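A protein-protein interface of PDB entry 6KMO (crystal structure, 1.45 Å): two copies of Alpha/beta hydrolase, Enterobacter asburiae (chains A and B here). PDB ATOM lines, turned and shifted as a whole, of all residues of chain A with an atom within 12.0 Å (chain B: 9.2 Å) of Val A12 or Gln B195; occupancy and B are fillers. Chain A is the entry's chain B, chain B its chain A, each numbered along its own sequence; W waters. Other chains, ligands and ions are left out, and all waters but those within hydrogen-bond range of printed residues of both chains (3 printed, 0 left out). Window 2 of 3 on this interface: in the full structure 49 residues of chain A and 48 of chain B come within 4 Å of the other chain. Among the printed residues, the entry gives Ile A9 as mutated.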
ATOM      1  N   THR A   3      13.748  -9.082   2.993  1.00  0.00           N
ATOM      2  CA  THR A   3      13.751 -10.099   4.034  1.00  0.00           C
ATOM      3  C   THR A   3      15.011 -10.947   3.918  1.00  0.00           C
ATOM      4  O   THR A   3      15.793 -11.049   4.864  1.00  0.00           O
ATOM      5  CB  THR A   3      12.523 -11.017   3.918  1.00  0.00           C
ATOM      6  OG1 THR A   3      11.333 -10.218   3.943  1.00  0.00           O
ATOM      7  CG2 THR A   3      12.480 -12.039   5.060  1.00  0.00           C
ATOM      8  N   LEU A   4      15.195 -11.571   2.749  1.00  0.00           N
ATOM      9  CA  LEU A   4      16.396 -12.373   2.538  1.00  0.00           C
ATOM     10  C   LEU A   4      17.640 -11.498   2.591  1.00  0.00           C
ATOM     11  O   LEU A   4      18.654 -11.869   3.196  1.00  0.00           O
ATOM     12  CB  LEU A   4      16.311 -13.123   1.198  1.00  0.00           C
ATOM     13  CG  LEU A   4      17.026 -14.481   1.210  1.00  0.00           C
ATOM     14  CD1 LEU A   4      17.000 -15.299  -0.080  1.00  0.00           C
ATOM     15  CD2 LEU A   4      18.440 -14.214   1.573  1.00  0.00           C
ATOM     16  N   THR A   5      17.585 -10.327   1.966  1.00  0.00           N
ATOM     17  CA  THR A   5      18.760  -9.469   1.883  1.00  0.00           C
ATOM     18  C   THR A   5      19.313  -9.140   3.268  1.00  0.00           C
ATOM     19  O   THR A   5      20.535  -9.046   3.437  1.00  0.00           O
ATOM     20  CB  THR A   5      18.416  -8.241   1.035  1.00  0.00           C
ATOM     21  OG1 THR A   5      18.368  -8.632  -0.349  1.00  0.00           O
ATOM     22  CG2 THR A   5      19.453  -7.157   1.204  1.00  0.00           C
ATOM     23  N   ALA A   6      18.454  -9.022   4.289  1.00  0.00           N
ATOM     24  CA  ALA A   6      18.972  -8.724   5.620  1.00  0.00           C
ATOM     25  C   ALA A   6      19.861  -9.851   6.132  1.00  0.00           C
ATOM     26  O   ALA A   6      20.918  -9.606   6.729  1.00  0.00           O
ATOM     27  CB  ALA A   6      17.823  -8.492   6.603  1.00  0.00           C
ATOM     28  N   ILE A   7      19.460 -11.094   5.900  1.00  0.00           N
ATOM     29  CA  ILE A   7      20.266 -12.224   6.327  1.00  0.00           C
ATOM     30  C   ILE A   7      21.542 -12.322   5.500  1.00  0.00           C
ATOM     31  O   ILE A   7      22.621 -12.619   6.035  1.00  0.00           O
ATOM     32  CB  ILE A   7      19.412 -13.501   6.284  1.00  0.00           C
ATOM     33  CG1 ILE A   7      18.235 -13.359   7.264  1.00  0.00           C
ATOM     34  CG2 ILE A   7      20.234 -14.688   6.615  1.00  0.00           C
ATOM     35  CD1 ILE A   7      17.018 -14.201   6.893  1.00  0.00           C
ATOM     36  N   LEU A   8      21.458 -12.030   4.193  1.00  0.00           N
ATOM     37  CA  LEU A   8      22.617 -12.207   3.323  1.00  0.00           C
ATOM     38  C   LEU A   8      23.751 -11.258   3.675  1.00  0.00           C
ATOM     39  O   LEU A   8      24.917 -11.606   3.466  1.00  0.00           O
ATOM     40  CB  LEU A   8      22.252 -12.016   1.854  1.00  0.00           C
ATOM     41  CG  LEU A   8      21.217 -12.999   1.326  1.00  0.00           C
ATOM     42  CD1 LEU A   8      20.868 -12.692  -0.137  1.00  0.00           C
ATOM     43  CD2 LEU A   8      21.634 -14.446   1.469  1.00  0.00           C
ATOM     44  N   ILE A   9      23.448 -10.064   4.185  1.00  0.00           N
ATOM     45  CA  ILE A   9      24.495  -9.113   4.528  1.00  0.00           C
ATOM     46  C   ILE A   9      24.959  -9.263   5.970  1.00  0.00           C
ATOM     47  O   ILE A   9      25.881  -8.552   6.396  1.00  0.00           O
ATOM     48  CB  ILE A   9      24.098  -7.652   4.240  1.00  0.00           C
ATOM     49  CG1 ILE A   9      22.909  -7.241   5.116  1.00  0.00           C
ATOM     50  CG2 ILE A   9      23.793  -7.452   2.761  1.00  0.00           C
ATOM     51  CD1 ILE A   9      22.632  -5.747   5.056  1.00  0.00           C
ATOM     52  N   SER A  10      24.374 -10.192   6.722  1.00  0.00           N
ATOM     53  CA  SER A  10      24.595 -10.281   8.153  1.00  0.00           C
ATOM     54  C   SER A  10      25.823 -11.102   8.513  1.00  0.00           C
ATOM     55  O   SER A  10      26.475 -11.728   7.671  1.00  0.00           O
ATOM     56  CB  SER A  10      23.380 -10.953   8.807  1.00  0.00           C
ATOM     57  OG  SER A  10      23.429 -12.368   8.666  1.00  0.00           O
ATOM     58  N   SER A  11      26.118 -11.141   9.806  1.00  0.00           N
ATOM     59  CA  SER A  11      27.237 -11.919  10.313  1.00  0.00           C
ATOM     60  C   SER A  11      27.091 -13.420  10.081  1.00  0.00           C
ATOM     61  O   SER A  11      28.082 -14.144  10.232  1.00  0.00           O
ATOM     62  CB  SER A  11      27.436 -11.618  11.789  1.00  0.00           C
ATOM     63  OG  SER A  11      26.286 -11.989  12.523  1.00  0.00           O
ATOM     64  N   VAL A  12      25.906 -13.905   9.711  1.00  0.00           N
ATOM     65  CA  VAL A  12      25.768 -15.313   9.345  1.00  0.00           C
ATOM     66  C   VAL A  12      26.835 -15.697   8.327  1.00  0.00           C
ATOM     67  O   VAL A  12      27.377 -16.807   8.355  1.00  0.00           O
ATOM     68  CB  VAL A  12      24.353 -15.583   8.798  1.00  0.00           C
ATOM     69  CG1 VAL A  12      24.237 -16.994   8.248  1.00  0.00           C
ATOM     70  CG2 VAL A  12      23.330 -15.359   9.898  1.00  0.00           C
ATOM     71  N   PHE A  13      27.153 -14.777   7.416  1.00  0.00           N
ATOM     72  CA  PHE A  13      28.043 -15.042   6.287  1.00  0.00           C
ATOM     73  C   PHE A  13      29.371 -14.322   6.400  1.00  0.00           C
ATOM     74  O   PHE A  13      30.138 -14.296   5.432  1.00  0.00           O
ATOM     75  CB  PHE A  13      27.322 -14.655   5.002  1.00  0.00           C
ATOM     76  CG  PHE A  13      26.122 -15.519   4.699  1.00  0.00           C
ATOM     77  CD1 PHE A  13      26.289 -16.810   4.233  1.00  0.00           C
ATOM     78  CD2 PHE A  13      24.827 -15.053   4.888  1.00  0.00           C
ATOM     79  CE1 PHE A  13      25.191 -17.615   3.944  1.00  0.00           C
ATOM     80  CE2 PHE A  13      23.732 -15.860   4.625  1.00  0.00           C
ATOM     81  CZ  PHE A  13      23.912 -17.137   4.140  1.00  0.00           C
ATOM     82  N   ALA A  14      29.700 -13.760   7.556  1.00  0.00           N
ATOM     83  CA  ALA A  14      31.010 -13.150   7.715  1.00  0.00           C
ATOM     84  C   ALA A  14      32.130 -14.181   7.651  1.00  0.00           C
ATOM     85  O   ALA A  14      32.009 -15.301   8.151  1.00  0.00           O
ATOM     86  CB  ALA A  14      31.087 -12.403   9.045  1.00  0.00           C
ATOM     87  N   SER A  15      33.251 -13.781   7.049  1.00  0.00           N
ATOM     88  CA  SER A  15      34.498 -14.507   7.205  1.00  0.00           C
ATOM     89  C   SER A  15      35.132 -14.197   8.572  1.00  0.00           C
ATOM     90  O   SER A  15      34.602 -13.434   9.374  1.00  0.00           O
ATOM     91  CB  SER A  15      35.488 -14.080   6.121  1.00  0.00           C
ATOM     92  OG  SER A  15      36.763 -14.620   6.443  1.00  0.00           O
ATOM     93  N   ALA A  16      36.328 -14.742   8.803  1.00  0.00           N
ATOM     94  CA  ALA A  16      37.163 -14.326   9.935  1.00  0.00           C
ATOM     95  C   ALA A  16      37.387 -12.813   9.917  1.00  0.00           C
ATOM     96  O   ALA A  16      37.576 -12.206   8.859  1.00  0.00           O
ATOM     97  CB  ALA A  16      38.505 -15.056   9.909  1.00  0.00           C
ATOM     98  N   TYR B 154      19.835 -17.208  -6.322  1.00  0.00           N
ATOM     99  CA  TYR B 154      19.413 -18.274  -5.417  1.00  0.00           C
ATOM    100  C   TYR B 154      17.916 -18.564  -5.556  1.00  0.00           C
ATOM    101  O   TYR B 154      17.502 -19.727  -5.625  1.00  0.00           O
ATOM    102  CB  TYR B 154      19.779 -17.961  -3.954  1.00  0.00           C
ATOM    103  CG  TYR B 154      19.229 -19.012  -3.025  1.00  0.00           C
ATOM    104  CD1 TYR B 154      19.822 -20.246  -2.920  1.00  0.00           C
ATOM    105  CD2 TYR B 154      18.056 -18.795  -2.332  1.00  0.00           C
ATOM    106  CE1 TYR B 154      19.305 -21.242  -2.112  1.00  0.00           C
ATOM    107  CE2 TYR B 154      17.522 -19.780  -1.529  1.00  0.00           C
ATOM    108  CZ  TYR B 154      18.154 -20.990  -1.420  1.00  0.00           C
ATOM    109  OH  TYR B 154      17.607 -21.957  -0.606  1.00  0.00           O
ATOM    110  N   ALA B 187      29.442 -19.984  -6.502  1.00  0.00           N
ATOM    111  CA  ALA B 187      29.813 -20.198  -5.107  1.00  0.00           C
ATOM    112  C   ALA B 187      28.818 -19.542  -4.155  1.00  0.00           C
ATOM    113  O   ALA B 187      28.454 -20.129  -3.125  1.00  0.00           O
ATOM    114  CB  ALA B 187      31.232 -19.668  -4.859  1.00  0.00           C
ATOM    115  N   SER B 188      28.351 -18.341  -4.488  1.00  0.00           N
ATOM    116  CA  SER B 188      27.431 -17.623  -3.615  1.00  0.00           C
ATOM    117  C   SER B 188      26.116 -18.368  -3.478  1.00  0.00           C
ATOM    118  O   SER B 188      25.538 -18.444  -2.382  1.00  0.00           O
ATOM    119  CB  SER B 188      27.206 -16.237  -4.202  1.00  0.00           C
ATOM    120  OG  SER B 188      26.571 -15.398  -3.274  1.00  0.00           O
ATOM    121  N   VAL B 189      25.607 -18.912  -4.581  1.00  0.00           N
ATOM    122  CA  VAL B 189      24.358 -19.669  -4.542  1.00  0.00           C
ATOM    123  C   VAL B 189      24.556 -20.975  -3.796  1.00  0.00           C
ATOM    124  O   VAL B 189      23.709 -21.377  -2.994  1.00  0.00           O
ATOM    125  CB  VAL B 189      23.828 -19.882  -5.969  1.00  0.00           C
ATOM    126  CG1 VAL B 189      22.681 -20.909  -5.995  1.00  0.00           C
ATOM    127  CG2 VAL B 189      23.352 -18.566  -6.546  1.00  0.00           C
ATOM    128  N   ALA B 190      25.681 -21.652  -4.024  1.00  0.00           N
ATOM    129  CA  ALA B 190      25.950 -22.889  -3.302  1.00  0.00           C
ATOM    130  C   ALA B 190      26.034 -22.649  -1.794  1.00  0.00           C
ATOM    131  O   ALA B 190      25.537 -23.463  -1.000  1.00  0.00           O
ATOM    132  CB  ALA B 190      27.223 -23.552  -3.827  1.00  0.00           C
ATOM    133  N   LEU B 191      26.649 -21.547  -1.373  1.00  0.00           N
ATOM    134  CA  LEU B 191      26.779 -21.261   0.058  1.00  0.00           C
ATOM    135  C   LEU B 191      25.439 -20.856   0.664  1.00  0.00           C
ATOM    136  O   LEU B 191      25.138 -21.216   1.809  1.00  0.00           O
ATOM    137  CB  LEU B 191      27.844 -20.197   0.286  1.00  0.00           C
ATOM    138  CG  LEU B 191      29.290 -20.639   0.037  1.00  0.00           C
ATOM    139  CD1 LEU B 191      30.220 -19.455  -0.083  1.00  0.00           C
ATOM    140  CD2 LEU B 191      29.757 -21.611   1.112  1.00  0.00           C
ATOM    141  N   GLN B 192      24.600 -20.138  -0.084  1.00  0.00           N
ATOM    142  CA  GLN B 192      23.245 -19.886   0.400  1.00  0.00           C
ATOM    143  C   GLN B 192      22.478 -21.196   0.532  1.00  0.00           C
ATOM    144  O   GLN B 192      21.797 -21.428   1.538  1.00  0.00           O
ATOM    145  CB  GLN B 192      22.508 -18.960  -0.563  1.00  0.00           C
ATOM    146  CG  GLN B 192      22.948 -17.512  -0.514  1.00  0.00           C
ATOM    147  CD  GLN B 192      22.256 -16.698  -1.576  1.00  0.00           C
ATOM    148  OE1 GLN B 192      21.104 -16.312  -1.419  1.00  0.00           O
ATOM    149  NE2 GLN B 192      22.939 -16.469  -2.685  1.00  0.00           N
ATOM    150  N   ALA B 193      22.562 -22.065  -0.470  1.00  0.00           N
ATOM    151  CA  ALA B 193      21.852 -23.340  -0.410  1.00  0.00           C
ATOM    152  C   ALA B 193      22.293 -24.168   0.793  1.00  0.00           C
ATOM    153  O   ALA B 193      21.467 -24.826   1.435  1.00  0.00           O
ATOM    154  CB  ALA B 193      22.029 -24.109  -1.718  1.00  0.00           C
ATOM    155  N   LYS B 194      23.578 -24.131   1.135  1.00  0.00           N
ATOM    156  CA  LYS B 194      24.030 -24.849   2.320  1.00  0.00           C
ATOM    157  C   LYS B 194      23.422 -24.242   3.577  1.00  0.00           C
ATOM    158  O   LYS B 194      22.900 -24.959   4.437  1.00  0.00           O
ATOM    159  CB  LYS B 194      25.555 -24.847   2.394  1.00  0.00           C
ATOM    160  CG  LYS B 194      26.104 -25.529   3.646  1.00  0.00           C
ATOM    161  CD  LYS B 194      27.508 -26.084   3.422  1.00  0.00           C
ATOM    162  CE  LYS B 194      28.501 -24.991   3.066  1.00  0.00           C
ATOM    163  NZ  LYS B 194      28.623 -23.957   4.133  1.00  0.00           N
ATOM    164  N   GLN B 195      23.444 -22.913   3.687  1.00  0.00           N
ATOM    165  CA  GLN B 195      22.904 -22.273   4.879  1.00  0.00           C
ATOM    166  C   GLN B 195      21.406 -22.509   5.018  1.00  0.00           C
ATOM    167  O   GLN B 195      20.898 -22.670   6.138  1.00  0.00           O
ATOM    168  CB  GLN B 195      23.208 -20.777   4.850  1.00  0.00           C
ATOM    169  CG  GLN B 195      22.998 -20.104   6.196  1.00  0.00           C
ATOM    170  CD  GLN B 195      23.934 -20.648   7.259  1.00  0.00           C
ATOM    171  OE1 GLN B 195      25.075 -21.020   6.968  1.00  0.00           O
ATOM    172  NE2 GLN B 195      23.460 -20.706   8.487  1.00  0.00           N
ATOM    173  N   PHE B 196      20.683 -22.546   3.902  1.00  0.00           N
ATOM    174  CA  PHE B 196      19.224 -22.615   3.912  1.00  0.00           C
ATOM    175  C   PHE B 196      18.695 -24.033   3.689  1.00  0.00           C
ATOM    176  O   PHE B 196      17.489 -24.205   3.465  1.00  0.00           O
ATOM    177  CB  PHE B 196      18.647 -21.654   2.866  1.00  0.00           C
ATOM    178  CG  PHE B 196      19.106 -20.225   3.019  1.00  0.00           C
ATOM    179  CD1 PHE B 196      19.309 -19.664   4.263  1.00  0.00           C
ATOM    180  CD2 PHE B 196      19.331 -19.440   1.896  1.00  0.00           C
ATOM    181  CE1 PHE B 196      19.726 -18.346   4.390  1.00  0.00           C
ATOM    182  CE2 PHE B 196      19.737 -18.130   2.014  1.00  0.00           C
ATOM    183  CZ  PHE B 196      19.948 -17.580   3.252  1.00  0.00           C
ATOM    184  N   ASN B 197      19.566 -25.039   3.728  1.00  0.00           N
ATOM    185  CA  ASN B 197      19.198 -26.453   3.585  1.00  0.00           C
ATOM    186  C   ASN B 197      18.444 -26.756   2.284  1.00  0.00           C
ATOM    187  O   ASN B 197      17.407 -27.424   2.270  1.00  0.00           O
ATOM    188  CB  ASN B 197      18.423 -26.964   4.805  1.00  0.00           C
ATOM    189  CG  ASN B 197      19.131 -26.655   6.110  1.00  0.00           C
ATOM    190  OD1 ASN B 197      20.212 -27.179   6.383  1.00  0.00           O
ATOM    191  ND2 ASN B 197      18.529 -25.789   6.917  1.00  0.00           N
ATOM    192  N   GLY B 198      19.000 -26.293   1.174  1.00  0.00           N
ATOM    193  CA  GLY B 198      18.555 -26.736  -0.131  1.00  0.00           C
ATOM    194  C   GLY B 198      18.499 -25.566  -1.081  1.00  0.00           C
ATOM    195  O   GLY B 198      18.654 -24.401  -0.686  1.00  0.00           O
ATOM    196  N   PRO B 199      18.283 -25.845  -2.358  1.00  0.00           N
ATOM    197  CA  PRO B 199      18.134 -27.167  -2.962  1.00  0.00           C
ATOM    198  C   PRO B 199      19.440 -27.930  -3.170  1.00  0.00           C
ATOM    199  O   PRO B 199      20.519 -27.317  -3.103  1.00  0.00           O
ATOM    200  CB  PRO B 199      17.514 -26.841  -4.325  1.00  0.00           C
ATOM    201  CG  PRO B 199      18.081 -25.544  -4.661  1.00  0.00           C
ATOM    202  CD  PRO B 199      18.162 -24.777  -3.361  1.00  0.00           C
ATOM    203  N   LYS B 200      19.331 -29.239  -3.392  1.00  0.00           N
ATOM    204  CA  LYS B 200      20.479 -30.081  -3.690  1.00  0.00           C
ATOM    205  C   LYS B 200      21.092 -29.694  -5.028  1.00  0.00           C
ATOM    206  O   LYS B 200      20.380 -29.460  -6.004  1.00  0.00           O
ATOM    207  CB  LYS B 200      20.049 -31.548  -3.761  1.00  0.00           C
ATOM    208  CG  LYS B 200      19.762 -32.233  -2.435  1.00  0.00           C
ATOM    209  CD  LYS B 200      20.565 -31.626  -1.293  1.00  0.00           C
ATOM    210  CE  LYS B 200      19.660 -30.875  -0.326  1.00  0.00           C
ATOM    211  NZ  LYS B 200      20.392 -30.410   0.887  1.00  0.00           N
ATOM    212  N   ASN B 249      34.129  -8.742   2.982  1.00  0.00           N
ATOM    213  CA  ASN B 249      34.546  -9.787   3.897  1.00  0.00           C
ATOM    214  C   ASN B 249      33.481 -10.861   4.089  1.00  0.00           C
ATOM    215  O   ASN B 249      33.678 -11.774   4.900  1.00  0.00           O
ATOM    216  CB  ASN B 249      34.922  -9.171   5.246  1.00  0.00           C
ATOM    217  CG  ASN B 249      35.924  -9.989   5.993  1.00  0.00           C
ATOM    218  OD1 ASN B 249      36.942 -10.429   5.433  1.00  0.00           O
ATOM    219  ND2 ASN B 249      35.648 -10.228   7.276  1.00  0.00           N
ATOM    220  N   ASN B 250      32.364 -10.758   3.378  1.00  0.00           N
ATOM    221  CA  ASN B 250      31.257 -11.707   3.436  1.00  0.00           C
ATOM    222  C   ASN B 250      31.557 -12.823   2.449  1.00  0.00           C
ATOM    223  O   ASN B 250      31.949 -12.554   1.311  1.00  0.00           O
ATOM    224  CB  ASN B 250      30.008 -10.917   3.034  1.00  0.00           C
ATOM    225  CG  ASN B 250      28.718 -11.703   3.091  1.00  0.00           C
ATOM    226  OD1 ASN B 250      28.616 -12.832   2.621  1.00  0.00           O
ATOM    227  ND2 ASN B 250      27.689 -11.068   3.642  1.00  0.00           N
ATOM    228  N   ILE B 251      31.408 -14.078   2.890  1.00  0.00           N
ATOM    229  CA  ILE B 251      31.759 -15.213   2.031  1.00  0.00           C
ATOM    230  C   ILE B 251      30.884 -15.311   0.781  1.00  0.00           C
ATOM    231  O   ILE B 251      31.263 -16.006  -0.174  1.00  0.00           O
ATOM    232  CB  ILE B 251      31.757 -16.555   2.797  1.00  0.00           C
ATOM    233  CG1 ILE B 251      30.343 -16.966   3.238  1.00  0.00           C
ATOM    234  CG2 ILE B 251      32.713 -16.483   3.969  1.00  0.00           C
ATOM    235  CD1 ILE B 251      30.298 -18.351   3.879  1.00  0.00           C
ATOM    236  N   LEU B 252      29.728 -14.648   0.757  1.00  0.00           N
ATOM    237  CA  LEU B 252      28.877 -14.637  -0.422  1.00  0.00           C
ATOM    238  C   LEU B 252      29.380 -13.664  -1.476  1.00  0.00           C
ATOM    239  O   LEU B 252      28.842 -13.646  -2.594  1.00  0.00           O
ATOM    240  CB  LEU B 252      27.436 -14.287  -0.049  1.00  0.00           C
ATOM    241  CG  LEU B 252      26.795 -15.221   0.973  1.00  0.00           C
ATOM    242  CD1 LEU B 252      25.351 -14.790   1.231  1.00  0.00           C
ATOM    243  CD2 LEU B 252      26.835 -16.677   0.537  1.00  0.00           C
ATOM    244  N   ALA B 261      35.538 -24.893   7.738  1.00  0.00           N
ATOM    245  CA  ALA B 261      34.225 -25.274   8.230  1.00  0.00           C
ATOM    246  C   ALA B 261      33.100 -24.675   7.392  1.00  0.00           C
ATOM    247  O   ALA B 261      32.060 -25.312   7.185  1.00  0.00           O
ATOM    248  CB  ALA B 261      34.094 -24.842   9.687  1.00  0.00           C
ATOM    249  N   GLN B 262      33.286 -23.445   6.909  1.00  0.00           N
ATOM    250  CA  GLN B 262      32.280 -22.807   6.073  1.00  0.00           C
ATOM    251  C   GLN B 262      32.172 -23.460   4.704  1.00  0.00           C
ATOM    252  O   GLN B 262      31.105 -23.407   4.094  1.00  0.00           O
ATOM    253  CB  GLN B 262      32.594 -21.324   5.928  1.00  0.00           C
ATOM    254  CG  GLN B 262      32.248 -20.528   7.197  1.00  0.00           C
ATOM    255  CD  GLN B 262      32.701 -19.093   7.136  1.00  0.00           C
ATOM    256  OE1 GLN B 262      33.841 -18.780   6.786  1.00  0.00           O
ATOM    257  NE2 GLN B 262      31.814 -18.191   7.527  1.00  0.00           N
ATOM    258  N   LEU B 263      33.246 -24.073   4.217  1.00  0.00           N
ATOM    259  CA  LEU B 263      33.239 -24.726   2.910  1.00  0.00           C
ATOM    260  C   LEU B 263      32.836 -26.192   2.967  1.00  0.00           C
ATOM    261  O   LEU B 263      32.506 -26.777   1.934  1.00  0.00           O
ATOM    262  CB  LEU B 263      34.610 -24.580   2.237  1.00  0.00           C
ATOM    263  CG  LEU B 263      34.988 -23.135   1.912  1.00  0.00           C
ATOM    264  CD1 LEU B 263      36.419 -23.055   1.418  1.00  0.00           C
ATOM    265  CD2 LEU B 263      34.006 -22.547   0.891  1.00  0.00           C
ATOM    266  N   LYS B 264      32.844 -26.812   4.143  1.00  0.00           N
ATOM    267  CA  LYS B 264      32.468 -28.215   4.228  1.00  0.00           C
ATOM    268  C   LYS B 264      31.069 -28.427   3.659  1.00  0.00           C
ATOM    269  O   LYS B 264      30.145 -27.658   3.931  1.00  0.00           O
ATOM    270  CB  LYS B 264      32.512 -28.670   5.688  1.00  0.00           C
ATOM    271  CG  LYS B 264      32.262 -30.156   5.871  1.00  0.00           C
ATOM    272  CD  LYS B 264      32.244 -30.544   7.355  1.00  0.00           C
ATOM    273  CE  LYS B 264      31.945 -32.032   7.533  1.00  0.00           C
ATOM    274  NZ  LYS B 264      32.474 -32.566   8.820  1.00  0.00           N
ATOM    275  N   GLY B 265      30.911 -29.462   2.838  1.00  0.00           N
ATOM    276  CA  GLY B 265      29.636 -29.761   2.232  1.00  0.00           C
ATOM    277  C   GLY B 265      29.328 -29.014   0.943  1.00  0.00           C
ATOM    278  O   GLY B 265      28.260 -29.223   0.364  1.00  0.00           O
ATOM    279  N   PHE B 266      30.232 -28.157   0.480  1.00  0.00           N
ATOM    280  CA  PHE B 266      30.056 -27.493  -0.812  1.00  0.00           C
ATOM    281  C   PHE B 266      29.881 -28.560  -1.894  1.00  0.00           C
ATOM    282  O   PHE B 266      30.443 -29.649  -1.798  1.00  0.00           O
ATOM    283  CB  PHE B 266      31.352 -26.722  -1.071  1.00  0.00           C
ATOM    284  CG  PHE B 266      31.297 -25.589  -2.088  1.00  0.00           C
ATOM    285  CD1 PHE B 266      30.834 -24.326  -1.747  1.00  0.00           C
ATOM    286  CD2 PHE B 266      31.826 -25.772  -3.359  1.00  0.00           C
ATOM    287  CE1 PHE B 266      30.865 -23.290  -2.662  1.00  0.00           C
ATOM    288  CE2 PHE B 266      31.862 -24.726  -4.282  1.00  0.00           C
ATOM    289  CZ  PHE B 266      31.384 -23.496  -3.933  1.00  0.00           C
HETATM  290  O   HOH W   1      38.538 -12.596   6.371  1.00  0.00           O
HETATM  291  O   HOH W   2      27.883  -8.128   4.340  1.00  0.00           O
HETATM  292  O   HOH W   3      28.973 -18.936   7.774  1.00  0.00           O
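No position is printed for both chains.
NE2 of Gln B262 sits at hydrogen-bond distance from O of Ala A14 (3.0 Å). The side-chain amide nitrogen of Asn B250 lies within hydrogen-bond range of the backbone carbonyl oxygen of Leu A8 (2.8 Å). O of Ala A16 lies within hydrogen-bond range of ND2 of Asn B249 (3.2 Å). The backbone NH of Ser A15 is in hydrogen-bond range of the backbone carbonyl oxygen of Asn B249. The backbone NH of Ile B251 sits at hydrogen-bond distance from the backbone carbonyl oxygen of Phe A13 (2.8 Å).
The backbone NH (N) of Leu B252 lies within hydrogen-bond range of the side-chain amide oxygen (OD1) of Asn B250 (2.8 Å). N of Val A12 lies close to OG of Ser A10, at 3.1 Å. The side-chain hydroxyl (OG) of Ser B188 is in hydrogen-bond range of the backbone carbonyl oxygen (O) of Leu B252, at 2.9 Å. O of Ser B188 lies within hydrogen-bond range of NE2 of Gln B192, at 3.3 Å. NZ of Lys B194 lies within hydrogen-bond range of O of Gln B262, at 2.5 Å.
No residue of chain B comes within 4 Å of Ser A10. No residue of chain B comes within 4 Å of Ser A11. Val A12 touches one residue of chain B. Of the printed residues of chain B, Phe A13 touches Gln B195 (3.7 Å), Asn B250 (3.3 Å), Ile B251 (2.8 Å) and Leu B252 (3.6 Å). Of the printed residues of chain B, Ala A16 touches Asn B249. No residue of chain A comes within 4 Å of Ala B193. Of the printed residues of chain A, Gln B195 touches Val A12 (3.8 Å) and Phe A13 (3.7 Å). No residue of chain A comes within 4 Å of Asn B197. Printed residues of chain A within 4 Å of Asn B249: Ala A14 (3.97 Å), Ser A15 (3.0 Å) and Ala A16 (3.2 Å). Of the printed residues of chain A, Ile B251 touches Phe A13. The nearest residue of chain B that does not touch Val A12 is Gln B262 (4.7 Å). The nearest printed residue of chain B that does not touch Leu A8 is Tyr B154 (6.6 Å).
Water W1 lies within hydrogen-bond range of the side-chain hydroxyl (OG) of Ser A15, the backbone carbonyl oxygen (O) of Ala A16 and the side-chain amide oxygen (OD1) of Asn B249. Water W3 lies within hydrogen-bond range of the backbone carbonyl oxygen of Val A12 (2.7 Å) and the side-chain amide nitrogen of Gln B262 (2.9 Å). Water W2 lies within hydrogen-bond range of the backbone carbonyl oxygen (O) of Ile A9 and the side-chain amide nitrogen (ND2) of Asn B250.
Among the printed residues, pairs that only touch across the chains: Phe A13 with Asn B250, Leu A8 with Gln B192, Phe A13 with Leu B252, Phe A13 with Gln B195, Leu A8 with Leu B252, Val A12 with Gln B195, Ile A9 with Asn B250, Ala A14 with Asn B249 and Leu A8 with Phe B196.
Of the 14 printed residues of chain A, 7 touch a printed residue of chain B. Hydrophobic or aromatic side chains of chain A within 4 Å of the printed part of chain B: Leu A8, Val A12 and Phe A13. Of the 25 printed residues of chain B, 8 touch a printed residue of chain A. Hydrophobic or aromatic side chains of chain B that line the printed part of chain A: Phe B196, Ile B251 and Leu B252.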
